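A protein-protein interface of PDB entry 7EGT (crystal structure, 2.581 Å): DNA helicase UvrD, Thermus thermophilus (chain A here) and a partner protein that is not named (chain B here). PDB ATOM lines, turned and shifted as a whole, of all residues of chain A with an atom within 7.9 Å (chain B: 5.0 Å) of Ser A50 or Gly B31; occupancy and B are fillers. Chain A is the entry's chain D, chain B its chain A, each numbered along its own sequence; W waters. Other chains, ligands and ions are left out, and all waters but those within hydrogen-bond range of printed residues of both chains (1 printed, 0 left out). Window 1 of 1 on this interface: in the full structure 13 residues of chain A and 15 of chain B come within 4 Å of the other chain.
Among the printed residues, pairs that only touch across the chains: Leu A49 with Gly B31 (3.2 Å), Tyr A53 with Ser B385 (3.2 Å), Tyr A53 with Gln B386 (3.4 Å), Ser A50 with Ser B385 (3.5 Å), Ala A54 with Asp B30 (3.6 Å), Phe A24 with Glu B32 (3.6 Å), Phe A24 with Asp B30 (3.7 Å), Asp A35 with Ser B385 (3.8 Å), Leu A49 with Glu B32 (3.9 Å), Tyr A53 with Gly B31 (3.9 Å), Arg A48 with Glu B32 (3.9 Å), Ser A50 with Gln B386 (3.98 Å) and Ala A54 with Gly B31 (3.98 Å).
N of Glu B32 sits at hydrogen-bond distance from O of Ala B27 (3.1 Å).
O of Leu B28 is in hydrogen-bond range of NE2 of Gln B386 (2.8 Å).
NE2 of Gln B386 lies within hydrogen-bond range of O of Glu B32.
OD2 of Asp A35 lies within hydrogen-bond range of OG of Ser A50 (2.6 Å).
O of Asp A35 lies within hydrogen-bond range of N of Leu A51, at 2.8 Å.
The backbone NH (N) of Lys A52 sits at hydrogen-bond distance from the side-chain carboxylate (OD1) of Asp A35, at 3.2 Å.
O of Asp B30 is in hydrogen-bond range of NE2 of His A21, 2.8 Å away.
The backbone NH (N) of Ser A50 lies within hydrogen-bond range of the backbone carbonyl oxygen (O) of Gly B31 (2.7 Å).
The side-chain carboxylate (OE2) of Glu B32 is in salt-bridge range of the side-chain amino group (NZ) of Lys A47, at 2.8 Å.
The guanidinium group (NE) of Arg B33 is in salt-bridge range of the side-chain carboxylate (OE2) of Glu A36 (2.7 Å).
N of Arg B33 lies within hydrogen-bond range of O of Arg A48 (3.0 Å).
The backbone carbonyl oxygen of Tyr A53 lies close to the backbone carbonyl oxygen of Arg B29.
Water W1 lies within hydrogen-bond range of OG of Ser B385 (2.9 Å) and OH of Tyr A53 (2.9 Å).
Ser A50 touches just these residues of chain B: Gly B31, Ser B385 and Gln B386.
Gly B31 touches four residues of chain A.
Printed residues of chain A within 4 Å of Glu B32: Phe A24, Lys A47, Arg A48 and Leu A49.
Printed residues of chain A within 4 Å of Gln B386: Ser A50 (3.98 Å) and Tyr A53 (3.4 Å).
Printed residues of chain A within 4 Å of Arg B29: Tyr A53.
Printed residues of chain B within 4 Å of His A21: Asp B30 (2.8 Å).
Of the printed residues of chain B, Phe A24 touches Asp B30 and Glu B32.
Pro A22 touches none of the printed residues of chain B.
Val A37 touches none of the printed residues of chain B.
The nearest printed residue of chain A that does not touch Gln B386 is Asp A35 (5.8 Å).
Of the 9 printed residues of chain B, 7 touch a printed residue of chain A.
Printed residues of chain B that touch a printed residue of chain A: Arg B29, Asp B30, Gly B31, Glu B32, Arg B33, Ser B385 and Gln B386.
Among the printed residues, 19 pairs touch across the chains.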
ATOM      1  N   HIS A  21     -17.093  28.032 -16.474  1.00  0.00           N
ATOM      2  CA  HIS A  21     -16.719  27.270 -17.645  1.00  0.00           C
ATOM      3  C   HIS A  21     -17.907  26.448 -18.121  1.00  0.00           C
ATOM      4  O   HIS A  21     -18.627  25.876 -17.293  1.00  0.00           O
ATOM      5  CB  HIS A  21     -15.543  26.346 -17.317  1.00  0.00           C
ATOM      6  CG  HIS A  21     -15.075  25.524 -18.472  1.00  0.00           C
ATOM      7  ND1 HIS A  21     -15.692  24.351 -18.850  1.00  0.00           N
ATOM      8  CD2 HIS A  21     -14.042  25.700 -19.326  1.00  0.00           C
ATOM      9  CE1 HIS A  21     -15.060  23.842 -19.890  1.00  0.00           C
ATOM     10  NE2 HIS A  21     -14.056  24.642 -20.200  1.00  0.00           N
ATOM     11  N   PRO A  22     -18.136  26.366 -19.439  1.00  0.00           N
ATOM     12  CA  PRO A  22     -19.392  25.773 -19.928  1.00  0.00           C
ATOM     13  C   PRO A  22     -19.609  24.350 -19.474  1.00  0.00           C
ATOM     14  O   PRO A  22     -20.763  23.924 -19.343  1.00  0.00           O
ATOM     15  CB  PRO A  22     -19.246  25.855 -21.453  1.00  0.00           C
ATOM     16  CG  PRO A  22     -18.242  26.922 -21.689  1.00  0.00           C
ATOM     17  CD  PRO A  22     -17.287  26.844 -20.543  1.00  0.00           C
ATOM     18  N   PHE A  24     -17.148  22.690 -16.920  1.00  0.00           N
ATOM     19  CA  PHE A  24     -16.600  22.484 -15.585  1.00  0.00           C
ATOM     20  C   PHE A  24     -17.298  23.303 -14.510  1.00  0.00           C
ATOM     21  O   PHE A  24     -17.071  23.050 -13.324  1.00  0.00           O
ATOM     22  CB  PHE A  24     -15.111  22.819 -15.559  1.00  0.00           C
ATOM     23  CG  PHE A  24     -14.313  22.065 -16.564  1.00  0.00           C
ATOM     24  CD1 PHE A  24     -14.566  20.725 -16.803  1.00  0.00           C
ATOM     25  CD2 PHE A  24     -13.319  22.699 -17.288  1.00  0.00           C
ATOM     26  CE1 PHE A  24     -13.834  20.025 -17.748  1.00  0.00           C
ATOM     27  CE2 PHE A  24     -12.584  22.005 -18.227  1.00  0.00           C
ATOM     28  CZ  PHE A  24     -12.842  20.665 -18.458  1.00  0.00           C
ATOM     29  N   GLY A  34       0.181  34.079 -20.594  1.00  0.00           N
ATOM     30  CA  GLY A  34      -0.150  34.239 -21.997  1.00  0.00           C
ATOM     31  C   GLY A  34      -1.531  33.721 -22.342  1.00  0.00           C
ATOM     32  O   GLY A  34      -2.535  34.183 -21.791  1.00  0.00           O
ATOM     33  N   ASP A  35      -1.595  32.757 -23.257  1.00  0.00           N
ATOM     34  CA  ASP A  35      -2.866  32.141 -23.603  1.00  0.00           C
ATOM     35  C   ASP A  35      -3.255  31.023 -22.647  1.00  0.00           C
ATOM     36  O   ASP A  35      -4.422  30.613 -22.636  1.00  0.00           O
ATOM     37  CB  ASP A  35      -2.813  31.613 -25.042  1.00  0.00           C
ATOM     38  CG  ASP A  35      -4.088  30.896 -25.450  1.00  0.00           C
ATOM     39  OD1 ASP A  35      -5.114  31.575 -25.683  1.00  0.00           O
ATOM     40  OD2 ASP A  35      -4.067  29.647 -25.518  1.00  0.00           O
ATOM     41  N   GLU A  36      -2.320  30.533 -21.836  1.00  0.00           N
ATOM     42  CA  GLU A  36      -2.603  29.474 -20.876  1.00  0.00           C
ATOM     43  C   GLU A  36      -3.171  30.071 -19.594  1.00  0.00           C
ATOM     44  O   GLU A  36      -2.591  31.001 -19.028  1.00  0.00           O
ATOM     45  CB  GLU A  36      -1.340  28.675 -20.560  1.00  0.00           C
ATOM     46  CG  GLU A  36      -1.573  27.505 -19.629  1.00  0.00           C
ATOM     47  CD  GLU A  36      -0.300  26.743 -19.332  1.00  0.00           C
ATOM     48  OE1 GLU A  36       0.358  27.061 -18.324  1.00  0.00           O
ATOM     49  OE2 GLU A  36       0.050  25.833 -20.110  1.00  0.00           O
ATOM     50  N   VAL A  37      -4.307  29.543 -19.148  1.00  0.00           N
ATOM     51  CA  VAL A  37      -4.897  29.914 -17.868  1.00  0.00           C
ATOM     52  C   VAL A  37      -5.090  28.647 -17.045  1.00  0.00           C
ATOM     53  O   VAL A  37      -5.578  27.630 -17.556  1.00  0.00           O
ATOM     54  CB  VAL A  37      -6.224  30.682 -18.040  1.00  0.00           C
ATOM     55  CG1 VAL A  37      -7.254  29.852 -18.794  1.00  0.00           C
ATOM     56  CG2 VAL A  37      -6.766  31.108 -16.690  1.00  0.00           C
ATOM     57  N   THR A  38      -4.675  28.697 -15.785  1.00  0.00           N
ATOM     58  CA  THR A  38      -4.855  27.593 -14.855  1.00  0.00           C
ATOM     59  C   THR A  38      -6.007  27.933 -13.924  1.00  0.00           C
ATOM     60  O   THR A  38      -5.949  28.934 -13.206  1.00  0.00           O
ATOM     61  CB  THR A  38      -3.577  27.337 -14.059  1.00  0.00           C
ATOM     62  OG1 THR A  38      -2.543  26.915 -14.953  1.00  0.00           O
ATOM     63  CG2 THR A  38      -3.809  26.261 -13.041  1.00  0.00           C
ATOM     64  N   LYS A  47      -7.270  22.711 -13.828  1.00  0.00           N
ATOM     65  CA  LYS A  47      -7.314  22.567 -15.283  1.00  0.00           C
ATOM     66  C   LYS A  47      -6.384  23.577 -15.939  1.00  0.00           C
ATOM     67  O   LYS A  47      -6.425  24.769 -15.620  1.00  0.00           O
ATOM     68  CB  LYS A  47      -8.728  22.762 -15.836  1.00  0.00           C
ATOM     69  CG  LYS A  47      -9.680  21.618 -15.582  1.00  0.00           C
ATOM     70  CD  LYS A  47      -9.216  20.346 -16.255  1.00  0.00           C
ATOM     71  CE  LYS A  47     -10.302  19.290 -16.205  1.00  0.00           C
ATOM     72  NZ  LYS A  47      -9.874  18.023 -16.869  1.00  0.00           N
ATOM     73  N   ARG A  48      -5.564  23.097 -16.867  1.00  0.00           N
ATOM     74  CA  ARG A  48      -4.675  23.938 -17.660  1.00  0.00           C
ATOM     75  C   ARG A  48      -5.355  24.166 -19.008  1.00  0.00           C
ATOM     76  O   ARG A  48      -5.471  23.237 -19.814  1.00  0.00           O
ATOM     77  CB  ARG A  48      -3.313  23.267 -17.825  1.00  0.00           C
ATOM     78  CG  ARG A  48      -2.151  24.217 -18.013  1.00  0.00           C
ATOM     79  CD  ARG A  48      -1.233  24.200 -16.802  1.00  0.00           C
ATOM     80  NE  ARG A  48      -0.606  22.898 -16.597  1.00  0.00           N
ATOM     81  CZ  ARG A  48      -0.027  22.523 -15.459  1.00  0.00           C
ATOM     82  NH1 ARG A  48      -0.003  23.354 -14.423  1.00  0.00           N
ATOM     83  NH2 ARG A  48       0.519  21.315 -15.354  1.00  0.00           N
ATOM     84  N   LEU A  49      -5.822  25.391 -19.246  1.00  0.00           N
ATOM     85  CA  LEU A  49      -6.706  25.673 -20.367  1.00  0.00           C
ATOM     86  C   LEU A  49      -6.087  26.671 -21.340  1.00  0.00           C
ATOM     87  O   LEU A  49      -5.160  27.416 -21.010  1.00  0.00           O
ATOM     88  CB  LEU A  49      -8.062  26.206 -19.879  1.00  0.00           C
ATOM     89  CG  LEU A  49      -8.869  25.278 -18.961  1.00  0.00           C
ATOM     90  CD1 LEU A  49     -10.265  25.840 -18.709  1.00  0.00           C
ATOM     91  CD2 LEU A  49      -8.950  23.875 -19.534  1.00  0.00           C
ATOM     92  N   SER A  50      -6.618  26.662 -22.562  1.00  0.00           N
ATOM     93  CA  SER A  50      -6.315  27.668 -23.573  1.00  0.00           C
ATOM     94  C   SER A  50      -7.418  28.720 -23.575  1.00  0.00           C
ATOM     95  O   SER A  50      -8.606  28.379 -23.641  1.00  0.00           O
ATOM     96  CB  SER A  50      -6.187  27.028 -24.955  1.00  0.00           C
ATOM     97  OG  SER A  50      -6.035  28.016 -25.959  1.00  0.00           O
ATOM     98  N   LEU A  51      -7.025  29.996 -23.495  1.00  0.00           N
ATOM     99  CA  LEU A  51      -8.012  31.062 -23.349  1.00  0.00           C
ATOM    100  C   LEU A  51      -8.866  31.214 -24.601  1.00  0.00           C
ATOM    101  O   LEU A  51     -10.072  31.476 -24.503  1.00  0.00           O
ATOM    102  CB  LEU A  51      -7.322  32.384 -23.004  1.00  0.00           C
ATOM    103  CG  LEU A  51      -7.030  32.631 -21.521  1.00  0.00           C
ATOM    104  CD1 LEU A  51      -6.192  33.880 -21.355  1.00  0.00           C
ATOM    105  CD2 LEU A  51      -8.320  32.736 -20.713  1.00  0.00           C
ATOM    106  N   LYS A  52      -8.260  31.060 -25.786  1.00  0.00           N
ATOM    107  CA  LYS A  52      -9.023  31.156 -27.028  1.00  0.00           C
ATOM    108  C   LYS A  52     -10.236  30.231 -27.011  1.00  0.00           C
ATOM    109  O   LYS A  52     -11.310  30.596 -27.503  1.00  0.00           O
ATOM    110  CB  LYS A  52      -8.137  30.821 -28.234  1.00  0.00           C
ATOM    111  CG  LYS A  52      -6.925  31.715 -28.456  1.00  0.00           C
ATOM    112  CD  LYS A  52      -5.986  31.069 -29.480  1.00  0.00           C
ATOM    113  CE  LYS A  52      -4.703  31.866 -29.697  1.00  0.00           C
ATOM    114  NZ  LYS A  52      -4.821  32.884 -30.784  1.00  0.00           N
ATOM    115  N   TYR A  53     -10.091  29.032 -26.439  1.00  0.00           N
ATOM    116  CA  TYR A  53     -11.099  27.993 -26.576  1.00  0.00           C
ATOM    117  C   TYR A  53     -11.820  27.628 -25.286  1.00  0.00           C
ATOM    118  O   TYR A  53     -12.799  26.876 -25.348  1.00  0.00           O
ATOM    119  CB  TYR A  53     -10.463  26.728 -27.168  1.00  0.00           C
ATOM    120  CG  TYR A  53      -9.707  27.017 -28.435  1.00  0.00           C
ATOM    121  CD1 TYR A  53     -10.378  27.234 -29.634  1.00  0.00           C
ATOM    122  CD2 TYR A  53      -8.323  27.103 -28.435  1.00  0.00           C
ATOM    123  CE1 TYR A  53      -9.691  27.512 -30.794  1.00  0.00           C
ATOM    124  CE2 TYR A  53      -7.627  27.382 -29.592  1.00  0.00           C
ATOM    125  CZ  TYR A  53      -8.317  27.584 -30.765  1.00  0.00           C
ATOM    126  OH  TYR A  53      -7.617  27.855 -31.913  1.00  0.00           O
ATOM    127  N   ALA A  54     -11.382  28.129 -24.129  1.00  0.00           N
ATOM    128  CA  ALA A  54     -12.024  27.735 -22.879  1.00  0.00           C
ATOM    129  C   ALA A  54     -13.456  28.253 -22.776  1.00  0.00           C
ATOM    130  O   ALA A  54     -14.286  27.634 -22.099  1.00  0.00           O
ATOM    131  CB  ALA A  54     -11.200  28.219 -21.687  1.00  0.00           C
ATOM    132  N   GLU A  55     -13.760  29.380 -23.426  1.00  0.00           N
ATOM    133  CA  GLU A  55     -15.086  30.004 -23.353  1.00  0.00           C
ATOM    134  C   GLU A  55     -15.427  30.406 -21.920  1.00  0.00           C
ATOM    135  O   GLU A  55     -16.576  30.310 -21.486  1.00  0.00           O
ATOM    136  CB  GLU A  55     -16.172  29.093 -23.937  1.00  0.00           C
ATOM    137  N   LEU A  56     -14.418  30.858 -21.178  1.00  0.00           N
ATOM    138  CA  LEU A  56     -14.639  31.269 -19.798  1.00  0.00           C
ATOM    139  C   LEU A  56     -15.494  32.527 -19.755  1.00  0.00           C
ATOM    140  O   LEU A  56     -15.282  33.462 -20.532  1.00  0.00           O
ATOM    141  CB  LEU A  56     -13.307  31.521 -19.085  1.00  0.00           C
ATOM    142  CG  LEU A  56     -12.405  30.325 -18.772  1.00  0.00           C
ATOM    143  CD1 LEU A  56     -11.076  30.802 -18.220  1.00  0.00           C
ATOM    144  CD2 LEU A  56     -13.072  29.348 -17.806  1.00  0.00           C
ATOM    145  N   ALA B  27     -12.480  17.333 -25.230  1.00  0.00           N
ATOM    146  CA  ALA B  27     -11.343  17.916 -24.528  1.00  0.00           C
ATOM    147  C   ALA B  27     -10.935  19.243 -25.155  1.00  0.00           C
ATOM    148  O   ALA B  27     -10.770  20.251 -24.455  1.00  0.00           O
ATOM    149  CB  ALA B  27     -10.174  16.930 -24.525  1.00  0.00           C
ATOM    150  N   LEU B  28     -10.800  19.271 -26.484  1.00  0.00           N
ATOM    151  CA  LEU B  28     -10.319  20.473 -27.158  1.00  0.00           C
ATOM    152  C   LEU B  28     -11.340  21.603 -27.091  1.00  0.00           C
ATOM    153  O   LEU B  28     -10.973  22.766 -26.878  1.00  0.00           O
ATOM    154  CB  LEU B  28      -9.957  20.141 -28.605  1.00  0.00           C
ATOM    155  CG  LEU B  28      -8.751  19.205 -28.726  1.00  0.00           C
ATOM    156  CD1 LEU B  28      -8.596  18.648 -30.144  1.00  0.00           C
ATOM    157  CD2 LEU B  28      -7.483  19.919 -28.269  1.00  0.00           C
ATOM    158  N   ARG B  29     -12.626  21.289 -27.253  1.00  0.00           N
ATOM    159  CA  ARG B  29     -13.639  22.331 -27.151  1.00  0.00           C
ATOM    160  C   ARG B  29     -13.799  22.828 -25.725  1.00  0.00           C
ATOM    161  O   ARG B  29     -14.286  23.942 -25.523  1.00  0.00           O
ATOM    162  CB  ARG B  29     -14.976  21.824 -27.690  1.00  0.00           C
ATOM    163  CG  ARG B  29     -15.003  21.689 -29.208  1.00  0.00           C
ATOM    164  CD  ARG B  29     -16.319  21.110 -29.692  1.00  0.00           C
ATOM    165  NE  ARG B  29     -16.396  21.086 -31.151  1.00  0.00           N
ATOM    166  CZ  ARG B  29     -17.283  20.375 -31.841  1.00  0.00           C
ATOM    167  NH1 ARG B  29     -18.174  19.616 -31.213  1.00  0.00           N
ATOM    168  NH2 ARG B  29     -17.273  20.414 -33.167  1.00  0.00           N
ATOM    169  N   ASP B  30     -13.407  22.022 -24.735  1.00  0.00           N
ATOM    170  CA  ASP B  30     -13.317  22.506 -23.366  1.00  0.00           C
ATOM    171  C   ASP B  30     -12.183  23.501 -23.203  1.00  0.00           C
ATOM    172  O   ASP B  30     -12.151  24.233 -22.208  1.00  0.00           O
ATOM    173  CB  ASP B  30     -13.100  21.343 -22.388  1.00  0.00           C
ATOM    174  CG  ASP B  30     -14.358  20.536 -22.137  1.00  0.00           C
ATOM    175  OD1 ASP B  30     -15.461  21.062 -22.386  1.00  0.00           O
ATOM    176  OD2 ASP B  30     -14.243  19.379 -21.675  1.00  0.00           O
ATOM    177  N   GLY B  31     -11.253  23.541 -24.146  1.00  0.00           N
ATOM    178  CA  GLY B  31     -10.085  24.370 -23.990  1.00  0.00           C
ATOM    179  C   GLY B  31      -8.922  23.699 -23.306  1.00  0.00           C
ATOM    180  O   GLY B  31      -7.951  24.386 -22.970  1.00  0.00           O
ATOM    181  N   GLU B  32      -8.990  22.385 -23.084  1.00  0.00           N
ATOM    182  CA  GLU B  32      -7.864  21.650 -22.522  1.00  0.00           C
ATOM    183  C   GLU B  32      -6.603  21.958 -23.316  1.00  0.00           C
ATOM    184  O   GLU B  32      -6.612  21.982 -24.549  1.00  0.00           O
ATOM    185  CB  GLU B  32      -8.142  20.143 -22.533  1.00  0.00           C
ATOM    186  CG  GLU B  32      -9.357  19.692 -21.724  1.00  0.00           C
ATOM    187  CD  GLU B  32      -9.039  19.349 -20.276  1.00  0.00           C
ATOM    188  OE1 GLU B  32      -7.906  19.623 -19.820  1.00  0.00           O
ATOM    189  OE2 GLU B  32      -9.934  18.799 -19.594  1.00  0.00           O
ATOM    190  N   ARG B  33      -5.527  22.234 -22.601  1.00  0.00           N
ATOM    191  CA  ARG B  33      -4.304  22.651 -23.262  1.00  0.00           C
ATOM    192  C   ARG B  33      -3.476  21.460 -23.717  1.00  0.00           C
ATOM    193  O   ARG B  33      -2.789  21.540 -24.743  1.00  0.00           O
ATOM    194  CB  ARG B  33      -3.503  23.549 -22.321  1.00  0.00           C
ATOM    195  CG  ARG B  33      -2.192  24.009 -22.876  1.00  0.00           C
ATOM    196  CD  ARG B  33      -1.995  25.486 -22.637  1.00  0.00           C
ATOM    197  NE  ARG B  33      -0.578  25.821 -22.707  1.00  0.00           N
ATOM    198  CZ  ARG B  33       0.110  25.926 -23.838  1.00  0.00           C
ATOM    199  NH1 ARG B  33       1.398  26.228 -23.804  1.00  0.00           N
ATOM    200  NH2 ARG B  33      -0.488  25.730 -25.005  1.00  0.00           N
ATOM    201  N   SER B 385      -1.543  26.864 -28.901  1.00  0.00           N
ATOM    202  CA  SER B 385      -2.645  26.956 -27.955  1.00  0.00           C
ATOM    203  C   SER B 385      -2.970  25.598 -27.342  1.00  0.00           C
ATOM    204  O   SER B 385      -3.079  25.480 -26.120  1.00  0.00           O
ATOM    205  CB  SER B 385      -3.887  27.532 -28.637  1.00  0.00           C
ATOM    206  OG  SER B 385      -4.493  26.556 -29.472  1.00  0.00           O
ATOM    207  N   GLN B 386      -3.125  24.572 -28.177  1.00  0.00           N
ATOM    208  CA  GLN B 386      -3.479  23.234 -27.729  1.00  0.00           C
ATOM    209  C   GLN B 386      -2.603  22.213 -28.431  1.00  0.00           C
ATOM    210  O   GLN B 386      -2.326  22.340 -29.624  1.00  0.00           O
ATOM    211  CB  GLN B 386      -4.946  22.921 -28.014  1.00  0.00           C
ATOM    212  CG  GLN B 386      -5.916  23.860 -27.347  1.00  0.00           C
ATOM    213  CD  GLN B 386      -7.331  23.622 -27.802  1.00  0.00           C
ATOM    214  OE1 GLN B 386      -7.655  23.850 -28.963  1.00  0.00           O
ATOM    215  NE2 GLN B 386      -8.185  23.143 -26.896  1.00  0.00           N
HETATM  216  O   HOH W   1      -4.717  28.101 -31.876  1.00  0.00           O
